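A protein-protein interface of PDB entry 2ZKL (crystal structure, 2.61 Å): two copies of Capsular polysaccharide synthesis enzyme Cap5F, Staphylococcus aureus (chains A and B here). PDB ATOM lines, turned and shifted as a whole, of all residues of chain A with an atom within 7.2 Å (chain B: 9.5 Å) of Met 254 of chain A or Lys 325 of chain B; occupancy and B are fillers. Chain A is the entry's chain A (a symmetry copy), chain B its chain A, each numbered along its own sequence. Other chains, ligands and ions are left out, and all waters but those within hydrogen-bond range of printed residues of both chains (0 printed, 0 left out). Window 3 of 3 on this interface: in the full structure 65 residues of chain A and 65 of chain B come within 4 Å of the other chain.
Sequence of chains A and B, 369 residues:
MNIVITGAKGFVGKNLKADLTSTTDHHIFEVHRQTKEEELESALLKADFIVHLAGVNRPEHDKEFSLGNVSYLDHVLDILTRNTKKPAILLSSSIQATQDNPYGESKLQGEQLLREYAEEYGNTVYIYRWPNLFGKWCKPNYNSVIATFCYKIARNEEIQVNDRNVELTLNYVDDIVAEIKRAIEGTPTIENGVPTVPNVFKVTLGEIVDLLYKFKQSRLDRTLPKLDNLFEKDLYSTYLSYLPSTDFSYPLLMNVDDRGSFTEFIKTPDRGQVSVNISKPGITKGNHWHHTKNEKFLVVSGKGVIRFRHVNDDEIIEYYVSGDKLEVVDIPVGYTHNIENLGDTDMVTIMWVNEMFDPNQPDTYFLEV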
ATOM      1  N   ARG A 222      -7.789  31.139  20.397  1.00  0.00           N
ATOM      2  CA  ARG A 222      -9.162  31.649  20.302  1.00  0.00           C
ATOM      3  C   ARG A 222      -9.243  33.179  20.412  1.00  0.00           C
ATOM      4  O   ARG A 222     -10.196  33.726  20.947  1.00  0.00           O
ATOM      5  CB  ARG A 222     -10.039  31.018  21.394  1.00  0.00           C
ATOM      6  CG  ARG A 222      -9.730  29.555  21.714  1.00  0.00           C
ATOM      7  CD  ARG A 222      -9.772  28.655  20.492  1.00  0.00           C
ATOM      8  NE  ARG A 222      -9.371  27.293  20.830  1.00  0.00           N
ATOM      9  CZ  ARG A 222      -9.008  26.370  19.941  1.00  0.00           C
ATOM     10  NH1 ARG A 222      -8.985  26.660  18.651  1.00  0.00           N
ATOM     11  NH2 ARG A 222      -8.673  25.150  20.340  1.00  0.00           N
ATOM     12  N   TYR A 250     -11.456  24.777  12.128  1.00  0.00           N
ATOM     13  CA  TYR A 250     -10.467  24.333  13.085  1.00  0.00           C
ATOM     14  C   TYR A 250     -11.174  23.732  14.299  1.00  0.00           C
ATOM     15  O   TYR A 250     -12.253  24.181  14.698  1.00  0.00           O
ATOM     16  CB  TYR A 250      -9.539  25.481  13.507  1.00  0.00           C
ATOM     17  CG  TYR A 250     -10.230  26.707  14.047  1.00  0.00           C
ATOM     18  CD1 TYR A 250     -10.834  27.624  13.188  1.00  0.00           C
ATOM     19  CD2 TYR A 250     -10.265  26.965  15.416  1.00  0.00           C
ATOM     20  CE1 TYR A 250     -11.450  28.773  13.679  1.00  0.00           C
ATOM     21  CE2 TYR A 250     -10.881  28.114  15.919  1.00  0.00           C
ATOM     22  CZ  TYR A 250     -11.471  29.015  15.042  1.00  0.00           C
ATOM     23  OH  TYR A 250     -12.065  30.159  15.520  1.00  0.00           O
ATOM     24  N   PRO A 251     -10.584  22.682  14.884  1.00  0.00           N
ATOM     25  CA  PRO A 251     -11.162  22.016  16.053  1.00  0.00           C
ATOM     26  C   PRO A 251     -10.970  22.824  17.329  1.00  0.00           C
ATOM     27  O   PRO A 251      -9.930  23.440  17.542  1.00  0.00           O
ATOM     28  CB  PRO A 251     -10.407  20.689  16.095  1.00  0.00           C
ATOM     29  CG  PRO A 251      -9.021  21.103  15.636  1.00  0.00           C
ATOM     30  CD  PRO A 251      -9.335  22.016  14.460  1.00  0.00           C
ATOM     31  N   LEU A 252     -11.991  22.820  18.170  1.00  0.00           N
ATOM     32  CA  LEU A 252     -11.950  23.523  19.445  1.00  0.00           C
ATOM     33  C   LEU A 252     -11.501  22.506  20.509  1.00  0.00           C
ATOM     34  O   LEU A 252     -11.630  21.295  20.302  1.00  0.00           O
ATOM     35  CB  LEU A 252     -13.352  24.054  19.763  1.00  0.00           C
ATOM     36  CG  LEU A 252     -13.583  25.557  19.976  1.00  0.00           C
ATOM     37  CD1 LEU A 252     -12.533  26.398  19.262  1.00  0.00           C
ATOM     38  CD2 LEU A 252     -14.992  25.884  19.499  1.00  0.00           C
ATOM     39  N   LEU A 253     -10.976  22.991  21.633  1.00  0.00           N
ATOM     40  CA  LEU A 253     -10.521  22.119  22.716  1.00  0.00           C
ATOM     41  C   LEU A 253     -11.634  21.787  23.709  1.00  0.00           C
ATOM     42  O   LEU A 253     -11.909  22.571  24.619  1.00  0.00           O
ATOM     43  CB  LEU A 253      -9.365  22.766  23.483  1.00  0.00           C
ATOM     44  CG  LEU A 253      -8.910  21.982  24.723  1.00  0.00           C
ATOM     45  CD1 LEU A 253      -8.421  20.591  24.304  1.00  0.00           C
ATOM     46  CD2 LEU A 253      -7.807  22.739  25.460  1.00  0.00           C
ATOM     47  N   MET A 254     -12.265  20.629  23.531  1.00  0.00           N
ATOM     48  CA  MET A 254     -13.336  20.183  24.428  1.00  0.00           C
ATOM     49  C   MET A 254     -12.797  19.516  25.698  1.00  0.00           C
ATOM     50  O   MET A 254     -12.025  18.573  25.616  1.00  0.00           O
ATOM     51  CB  MET A 254     -14.250  19.169  23.727  1.00  0.00           C
ATOM     52  CG  MET A 254     -15.227  19.739  22.727  1.00  0.00           C
ATOM     53  SD  MET A 254     -16.299  18.446  22.035  1.00  0.00           S
ATOM     54  CE  MET A 254     -15.215  17.790  20.905  1.00  0.00           C
ATOM     55  N   ASN A 255     -13.186  20.015  26.865  1.00  0.00           N
ATOM     56  CA  ASN A 255     -12.778  19.389  28.128  1.00  0.00           C
ATOM     57  C   ASN A 255     -13.926  18.422  28.412  1.00  0.00           C
ATOM     58  O   ASN A 255     -15.047  18.846  28.721  1.00  0.00           O
ATOM     59  CB  ASN A 255     -12.686  20.401  29.274  1.00  0.00           C
ATOM     60  CG  ASN A 255     -11.568  21.400  29.087  1.00  0.00           C
ATOM     61  OD1 ASN A 255     -11.556  22.168  28.119  1.00  0.00           O
ATOM     62  ND2 ASN A 255     -10.622  21.407  30.021  1.00  0.00           N
ATOM     63  N   VAL A 256     -13.648  17.130  28.292  1.00  0.00           N
ATOM     64  CA  VAL A 256     -14.671  16.116  28.493  1.00  0.00           C
ATOM     65  C   VAL A 256     -14.529  15.270  29.753  1.00  0.00           C
ATOM     66  O   VAL A 256     -13.424  15.010  30.229  1.00  0.00           O
ATOM     67  CB  VAL A 256     -14.711  15.167  27.277  1.00  0.00           C
ATOM     68  CG1 VAL A 256     -15.863  14.190  27.403  1.00  0.00           C
ATOM     69  CG2 VAL A 256     -14.834  15.980  25.999  1.00  0.00           C
ATOM     70  N   ASP A 257     -15.672  14.857  30.292  1.00  0.00           N
ATOM     71  CA  ASP A 257     -15.720  13.985  31.458  1.00  0.00           C
ATOM     72  C   ASP A 257     -17.119  13.372  31.571  1.00  0.00           C
ATOM     73  O   ASP A 257     -17.873  13.356  30.593  1.00  0.00           O
ATOM     74  CB  ASP A 257     -15.334  14.739  32.737  1.00  0.00           C
ATOM     75  CG  ASP A 257     -16.423  15.657  33.239  1.00  0.00           C
ATOM     76  OD1 ASP A 257     -17.558  15.618  32.715  1.00  0.00           O
ATOM     77  OD2 ASP A 257     -16.137  16.421  34.182  1.00  0.00           O
ATOM     78  N   GLY A 260     -20.193  15.875  31.147  1.00  0.00           N
ATOM     79  CA  GLY A 260     -20.373  16.401  29.808  1.00  0.00           C
ATOM     80  C   GLY A 260     -19.099  17.062  29.317  1.00  0.00           C
ATOM     81  O   GLY A 260     -18.039  16.429  29.298  1.00  0.00           O
ATOM     82  N   SER A 261     -19.179  18.333  28.930  1.00  0.00           N
ATOM     83  CA  SER A 261     -17.990  19.022  28.441  1.00  0.00           C
ATOM     84  C   SER A 261     -18.060  20.527  28.546  1.00  0.00           C
ATOM     85  O   SER A 261     -19.139  21.117  28.626  1.00  0.00           O
ATOM     86  CB  SER A 261     -17.726  18.660  26.977  1.00  0.00           C
ATOM     87  OG  SER A 261     -18.758  19.167  26.144  1.00  0.00           O
ATOM     88  N   PHE A 262     -16.883  21.137  28.528  1.00  0.00           N
ATOM     89  CA  PHE A 262     -16.754  22.581  28.580  1.00  0.00           C
ATOM     90  C   PHE A 262     -15.728  22.981  27.512  1.00  0.00           C
ATOM     91  O   PHE A 262     -14.581  22.521  27.530  1.00  0.00           O
ATOM     92  CB  PHE A 262     -16.302  23.017  29.970  1.00  0.00           C
ATOM     93  CG  PHE A 262     -16.331  24.498  30.172  1.00  0.00           C
ATOM     94  CD1 PHE A 262     -15.224  25.279  29.854  1.00  0.00           C
ATOM     95  CD2 PHE A 262     -17.481  25.122  30.650  1.00  0.00           C
ATOM     96  CE1 PHE A 262     -15.259  26.663  30.008  1.00  0.00           C
ATOM     97  CE2 PHE A 262     -17.529  26.510  30.809  1.00  0.00           C
ATOM     98  CZ  PHE A 262     -16.413  27.279  30.488  1.00  0.00           C
ATOM     99  N   THR A 263     -16.140  23.843  26.589  1.00  0.00           N
ATOM    100  CA  THR A 263     -15.264  24.259  25.495  1.00  0.00           C
ATOM    101  C   THR A 263     -15.118  25.772  25.330  1.00  0.00           C
ATOM    102  O   THR A 263     -16.117  26.493  25.281  1.00  0.00           O
ATOM    103  CB  THR A 263     -15.798  23.701  24.155  1.00  0.00           C
ATOM    104  OG1 THR A 263     -15.983  22.287  24.268  1.00  0.00           O
ATOM    105  CG2 THR A 263     -14.837  24.000  23.021  1.00  0.00           C
ATOM    106  N   GLU A 264     -13.886  26.260  25.233  1.00  0.00           N
ATOM    107  CA  GLU A 264     -13.691  27.693  25.012  1.00  0.00           C
ATOM    108  C   GLU A 264     -13.886  27.989  23.524  1.00  0.00           C
ATOM    109  O   GLU A 264     -13.418  27.244  22.661  1.00  0.00           O
ATOM    110  CB  GLU A 264     -12.297  28.144  25.452  1.00  0.00           C
ATOM    111  CG  GLU A 264     -12.107  28.101  26.944  1.00  0.00           C
ATOM    112  CD  GLU A 264     -10.707  28.476  27.352  1.00  0.00           C
ATOM    113  OE1 GLU A 264      -9.755  28.072  26.644  1.00  0.00           O
ATOM    114  OE2 GLU A 264     -10.560  29.162  28.389  1.00  0.00           O
ATOM    115  N   VAL A 276     -18.698  27.178  25.696  1.00  0.00           N
ATOM    116  CA  VAL A 276     -19.886  26.357  25.550  1.00  0.00           C
ATOM    117  C   VAL A 276     -19.867  25.207  26.553  1.00  0.00           C
ATOM    118  O   VAL A 276     -18.952  24.369  26.547  1.00  0.00           O
ATOM    119  CB  VAL A 276     -19.981  25.782  24.126  1.00  0.00           C
ATOM    120  CG1 VAL A 276     -21.236  24.937  23.982  1.00  0.00           C
ATOM    121  CG2 VAL A 276     -19.989  26.909  23.124  1.00  0.00           C
ATOM    122  N   ILE A 278     -21.715  21.841  28.035  1.00  0.00           N
ATOM    123  CA  ILE A 278     -22.692  20.817  27.707  1.00  0.00           C
ATOM    124  C   ILE A 278     -22.834  19.900  28.910  1.00  0.00           C
ATOM    125  O   ILE A 278     -21.851  19.355  29.401  1.00  0.00           O
ATOM    126  CB  ILE A 278     -22.278  20.009  26.455  1.00  0.00           C
ATOM    127  CG1 ILE A 278     -22.111  20.964  25.270  1.00  0.00           C
ATOM    128  CG2 ILE A 278     -23.353  18.969  26.119  1.00  0.00           C
ATOM    129  CD1 ILE A 278     -21.645  20.303  23.992  1.00  0.00           C
ATOM    130  N   PHE B 297     -18.841  30.206  12.511  1.00  0.00           N
ATOM    131  CA  PHE B 297     -19.997  29.375  12.836  1.00  0.00           C
ATOM    132  C   PHE B 297     -19.572  28.220  13.752  1.00  0.00           C
ATOM    133  O   PHE B 297     -18.552  27.580  13.514  1.00  0.00           O
ATOM    134  CB  PHE B 297     -20.618  28.773  11.568  1.00  0.00           C
ATOM    135  CG  PHE B 297     -21.403  29.748  10.729  1.00  0.00           C
ATOM    136  CD1 PHE B 297     -21.535  31.080  11.100  1.00  0.00           C
ATOM    137  CD2 PHE B 297     -22.026  29.317   9.553  1.00  0.00           C
ATOM    138  CE1 PHE B 297     -22.274  31.965  10.315  1.00  0.00           C
ATOM    139  CE2 PHE B 297     -22.766  30.195   8.764  1.00  0.00           C
ATOM    140  CZ  PHE B 297     -22.890  31.521   9.145  1.00  0.00           C
ATOM    141  N   LEU B 298     -20.356  27.967  14.794  1.00  0.00           N
ATOM    142  CA  LEU B 298     -20.080  26.876  15.727  1.00  0.00           C
ATOM    143  C   LEU B 298     -21.399  26.189  16.083  1.00  0.00           C
ATOM    144  O   LEU B 298     -22.228  26.767  16.791  1.00  0.00           O
ATOM    145  CB  LEU B 298     -19.423  27.416  16.995  1.00  0.00           C
ATOM    146  CG  LEU B 298     -19.171  26.406  18.116  1.00  0.00           C
ATOM    147  CD1 LEU B 298     -18.176  25.353  17.664  1.00  0.00           C
ATOM    148  CD2 LEU B 298     -18.639  27.147  19.348  1.00  0.00           C
ATOM    149  N   VAL B 299     -21.615  24.974  15.586  1.00  0.00           N
ATOM    150  CA  VAL B 299     -22.864  24.292  15.900  1.00  0.00           C
ATOM    151  C   VAL B 299     -22.702  23.515  17.204  1.00  0.00           C
ATOM    152  O   VAL B 299     -21.786  22.713  17.362  1.00  0.00           O
ATOM    153  CB  VAL B 299     -23.328  23.373  14.748  1.00  0.00           C
ATOM    154  CG1 VAL B 299     -23.172  24.100  13.423  1.00  0.00           C
ATOM    155  CG2 VAL B 299     -22.566  22.087  14.751  1.00  0.00           C
ATOM    156  N   VAL B 300     -23.598  23.790  18.145  1.00  0.00           N
ATOM    157  CA  VAL B 300     -23.548  23.180  19.462  1.00  0.00           C
ATOM    158  C   VAL B 300     -24.642  22.143  19.702  1.00  0.00           C
ATOM    159  O   VAL B 300     -24.701  21.527  20.762  1.00  0.00           O
ATOM    160  CB  VAL B 300     -23.618  24.284  20.552  1.00  0.00           C
ATOM    161  CG1 VAL B 300     -22.388  25.182  20.448  1.00  0.00           C
ATOM    162  CG2 VAL B 300     -24.897  25.119  20.390  1.00  0.00           C
ATOM    163  N   SER B 301     -25.502  21.952  18.713  1.00  0.00           N
ATOM    164  CA  SER B 301     -26.584  20.983  18.816  1.00  0.00           C
ATOM    165  C   SER B 301     -27.191  20.738  17.444  1.00  0.00           C
ATOM    166  O   SER B 301     -27.508  21.679  16.707  1.00  0.00           O
ATOM    167  CB  SER B 301     -27.661  21.482  19.780  1.00  0.00           C
ATOM    168  OG  SER B 301     -28.833  20.689  19.696  1.00  0.00           O
ATOM    169  N   GLY B 302     -27.360  19.464  17.114  1.00  0.00           N
ATOM    170  CA  GLY B 302     -27.903  19.107  15.821  1.00  0.00           C
ATOM    171  C   GLY B 302     -26.747  18.801  14.889  1.00  0.00           C
ATOM    172  O   GLY B 302     -25.597  18.665  15.330  1.00  0.00           O
ATOM    173  N   LYS B 303     -27.042  18.689  13.601  1.00  0.00           N
ATOM    174  CA  LYS B 303     -26.014  18.397  12.612  1.00  0.00           C
ATOM    175  C   LYS B 303     -26.476  18.925  11.262  1.00  0.00           C
ATOM    176  O   LYS B 303     -27.679  18.990  10.994  1.00  0.00           O
ATOM    177  CB  LYS B 303     -25.764  16.888  12.525  1.00  0.00           C
ATOM    178  CG  LYS B 303     -26.979  16.097  12.073  1.00  0.00           C
ATOM    179  CD  LYS B 303     -26.673  14.619  11.845  1.00  0.00           C
ATOM    180  CE  LYS B 303     -27.921  13.907  11.315  1.00  0.00           C
ATOM    181  NZ  LYS B 303     -27.754  12.435  11.132  1.00  0.00           N
ATOM    182  N   TYR B 320     -19.256  19.253   6.708  1.00  0.00           N
ATOM    183  CA  TYR B 320     -20.259  18.552   7.507  1.00  0.00           C
ATOM    184  C   TYR B 320     -19.866  18.725   8.962  1.00  0.00           C
ATOM    185  O   TYR B 320     -18.717  18.463   9.342  1.00  0.00           O
ATOM    186  CB  TYR B 320     -20.330  17.068   7.116  1.00  0.00           C
ATOM    187  CG  TYR B 320     -20.946  16.881   5.757  1.00  0.00           C
ATOM    188  CD1 TYR B 320     -20.159  16.882   4.608  1.00  0.00           C
ATOM    189  CD2 TYR B 320     -22.332  16.815   5.610  1.00  0.00           C
ATOM    190  CE1 TYR B 320     -20.736  16.833   3.343  1.00  0.00           C
ATOM    191  CE2 TYR B 320     -22.922  16.768   4.354  1.00  0.00           C
ATOM    192  CZ  TYR B 320     -22.118  16.782   3.218  1.00  0.00           C
ATOM    193  OH  TYR B 320     -22.704  16.783   1.965  1.00  0.00           O
ATOM    194  N   VAL B 321     -20.823  19.151   9.778  1.00  0.00           N
ATOM    195  CA  VAL B 321     -20.523  19.430  11.173  1.00  0.00           C
ATOM    196  C   VAL B 321     -21.706  19.201  12.114  1.00  0.00           C
ATOM    197  O   VAL B 321     -22.861  19.237  11.679  1.00  0.00           O
ATOM    198  CB  VAL B 321     -20.051  20.895  11.272  1.00  0.00           C
ATOM    199  CG1 VAL B 321     -21.222  21.832  10.942  1.00  0.00           C
ATOM    200  CG2 VAL B 321     -19.455  21.169  12.633  1.00  0.00           C
ATOM    201  N   SER B 322     -21.421  18.969  13.399  1.00  0.00           N
ATOM    202  CA  SER B 322     -22.482  18.753  14.391  1.00  0.00           C
ATOM    203  C   SER B 322     -22.040  19.009  15.831  1.00  0.00           C
ATOM    204  O   SER B 322     -20.866  19.229  16.107  1.00  0.00           O
ATOM    205  CB  SER B 322     -23.027  17.326  14.302  1.00  0.00           C
ATOM    206  OG  SER B 322     -22.213  16.440  15.051  1.00  0.00           O
ATOM    207  N   GLY B 323     -23.002  18.948  16.747  1.00  0.00           N
ATOM    208  CA  GLY B 323     -22.724  19.180  18.154  1.00  0.00           C
ATOM    209  C   GLY B 323     -21.868  18.143  18.866  1.00  0.00           C
ATOM    210  O   GLY B 323     -21.408  18.390  19.985  1.00  0.00           O
ATOM    211  N   ASP B 324     -21.644  16.988  18.244  1.00  0.00           N
ATOM    212  CA  ASP B 324     -20.829  15.957  18.883  1.00  0.00           C
ATOM    213  C   ASP B 324     -19.375  16.394  18.962  1.00  0.00           C
ATOM    214  O   ASP B 324     -18.736  16.244  20.001  1.00  0.00           O
ATOM    215  CB  ASP B 324     -20.945  14.630  18.130  1.00  0.00           C
ATOM    216  CG  ASP B 324     -22.387  14.176  17.984  1.00  0.00           C
ATOM    217  OD1 ASP B 324     -23.122  14.219  18.996  1.00  0.00           O
ATOM    218  OD2 ASP B 324     -22.787  13.778  16.863  1.00  0.00           O
ATOM    219  N   LYS B 325     -18.851  16.931  17.863  1.00  0.00           N
ATOM    220  CA  LYS B 325     -17.470  17.414  17.835  1.00  0.00           C
ATOM    221  C   LYS B 325     -17.515  18.924  17.607  1.00  0.00           C
ATOM    222  O   LYS B 325     -17.924  19.381  16.545  1.00  0.00           O
ATOM    223  CB  LYS B 325     -16.672  16.748  16.709  1.00  0.00           C
ATOM    224  CG  LYS B 325     -15.214  17.196  16.679  1.00  0.00           C
ATOM    225  CD  LYS B 325     -14.531  16.909  15.352  1.00  0.00           C
ATOM    226  CE  LYS B 325     -13.105  17.450  15.363  1.00  0.00           C
ATOM    227  NZ  LYS B 325     -12.402  17.243  14.062  1.00  0.00           N
ATOM    228  N   LEU B 326     -17.093  19.690  18.606  1.00  0.00           N
ATOM    229  CA  LEU B 326     -17.113  21.149  18.529  1.00  0.00           C
ATOM    230  C   LEU B 326     -15.995  21.765  17.694  1.00  0.00           C
ATOM    231  O   LEU B 326     -14.834  21.810  18.099  1.00  0.00           O
ATOM    232  CB  LEU B 326     -17.108  21.736  19.941  1.00  0.00           C
ATOM    233  CG  LEU B 326     -18.478  22.184  20.465  1.00  0.00           C
ATOM    234  CD1 LEU B 326     -19.593  21.318  19.900  1.00  0.00           C
ATOM    235  CD2 LEU B 326     -18.463  22.140  21.983  1.00  0.00           C
ATOM    236  N   GLU B 327     -16.361  22.244  16.513  1.00  0.00           N
ATOM    237  CA  GLU B 327     -15.382  22.845  15.632  1.00  0.00           C
ATOM    238  C   GLU B 327     -15.927  24.101  14.965  1.00  0.00           C
ATOM    239  O   GLU B 327     -17.076  24.145  14.506  1.00  0.00           O
ATOM    240  CB  GLU B 327     -14.912  21.821  14.589  1.00  0.00           C
ATOM    241  CG  GLU B 327     -15.950  21.388  13.574  1.00  0.00           C
ATOM    242  CD  GLU B 327     -15.532  20.125  12.820  1.00  0.00           C
ATOM    243  OE1 GLU B 327     -14.319  19.943  12.553  1.00  0.00           O
ATOM    244  OE2 GLU B 327     -16.425  19.316  12.485  1.00  0.00           O
ATOM    245  N   VAL B 328     -15.091  25.135  14.953  1.00  0.00           N
ATOM    246  CA  VAL B 328     -15.443  26.413  14.361  1.00  0.00           C
ATOM    247  C   VAL B 328     -15.171  26.396  12.868  1.00  0.00           C
ATOM    248  O   VAL B 328     -14.189  25.809  12.412  1.00  0.00           O
ATOM    249  CB  VAL B 328     -14.610  27.564  14.970  1.00  0.00           C
ATOM    250  CG1 VAL B 328     -14.932  28.881  14.244  1.00  0.00           C
ATOM    251  CG2 VAL B 328     -14.884  27.684  16.458  1.00  0.00           C
ATOM    252  N   VAL B 329     -16.055  27.030  12.110  1.00  0.00           N
ATOM    253  CA  VAL B 329     -15.888  27.145  10.669  1.00  0.00           C
ATOM    254  C   VAL B 329     -15.877  28.637  10.324  1.00  0.00           C
ATOM    255  O   VAL B 329     -16.891  29.324  10.484  1.00  0.00           O
ATOM    256  CB  VAL B 329     -17.043  26.481   9.896  1.00  0.00           C
ATOM    257  CG1 VAL B 329     -16.759  26.543   8.409  1.00  0.00           C
ATOM    258  CG2 VAL B 329     -17.220  25.039  10.344  1.00  0.00           C
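Met 254 of chain A touches just these residues of chain B: Asp 324 (3.9 Å), Lys 325 (3.8 Å) and Leu 326 (3.5 Å). Of chain A, only Met 254 comes within 4 Å of Lys 325 of chain B. Asn 255 of chain A touches none of the printed residues of chain B. Of the printed residues of chain A, Asp 324 of chain B touches Met 254 (3.9 Å). Printed residues of chain A within 4 Å of Leu 326 of chain B: Leu 252 (3.0 Å), Met 254 (3.5 Å) and Thr 263 (3.4 Å). Printed residues of chain A within 4 Å of Val 300 of chain B: Val 276 (3.7 Å). Printed residues of chain B within 4 Å of Val 276 of chain A: Val 300 (3.7 Å). Printed residues of chain B within 4 Å of Thr 263 of chain A: Leu 326. Val 329 of chain B touches none of the printed residues of chain A. Gly 323 of chain B touches none of the printed residues of chain A. The nearest residue of chain B that does not touch Met 254 of chain A is Gly 323 of chain B (5.5 Å). The nearest printed residue of chain A that does not touch Val 328 of chain B is Pro 251 of chain A (5.1 Å).
Hydrophobic or aromatic side chains of chain B that line the printed part of chain A: Leu 298, Val 300, Leu 326 and Val 328. Of the 16 printed residues of chain A, 5 touch a printed residue of chain B. Among the printed residues, no Asp or Glu carboxylate lies within 4 Å of a Lys or Arg side-chain nitrogen of the other chain.
The backbone carbonyl oxygen (O) of Val 328 of chain B lies within hydrogen-bond range of the backbone NH (N) of Tyr 250 of chain A (2.9 Å). The side-chain sulfur of Met 254 of chain A sits close to the backbone NH of Leu 326 of chain B (3.7 Å). The backbone NH (N) of Leu 252 of chain A sits at hydrogen-bond distance from the backbone carbonyl oxygen (O) of Leu 326 of chain B (3.0 Å).
No position is printed for both chains. Of the 10 pairs that touch across the chains among the printed residues, none has its exchanged pair printed and touching as well.
Among the printed residues, pairs that only touch across the chains: Tyr 250 of chain A with Glu 327 of chain B (3.5 Å), Leu 252 of chain A with Leu 298 of chain B (3.7 Å), Leu 252 of chain A with Val 328 of chain B (3.5 Å), Met 254 of chain A with Asp 324 of chain B (3.9 Å), Met 254 of chain A with Lys 325 of chain B (3.8 Å), Thr 263 of chain A with Leu 326 of chain B (3.4 Å) and Val 276 of chain A with Val 300 of chain B (3.7 Å).
The side-chain hydroxyl (OG) of Ser 322 of chain B is in hydrogen-bond range of the side-chain carboxylate (OD2) of Asp 324 of chain B. The backbone NH (N) of Val 276 of chain A lies within hydrogen-bond range of the backbone carbonyl oxygen (O) of Thr 263 of chain A. The side-chain amino group of Lys 325 of chain B is in salt-bridge range of the side-chain carboxylate of Glu 327 of chain B (3.6 Å).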
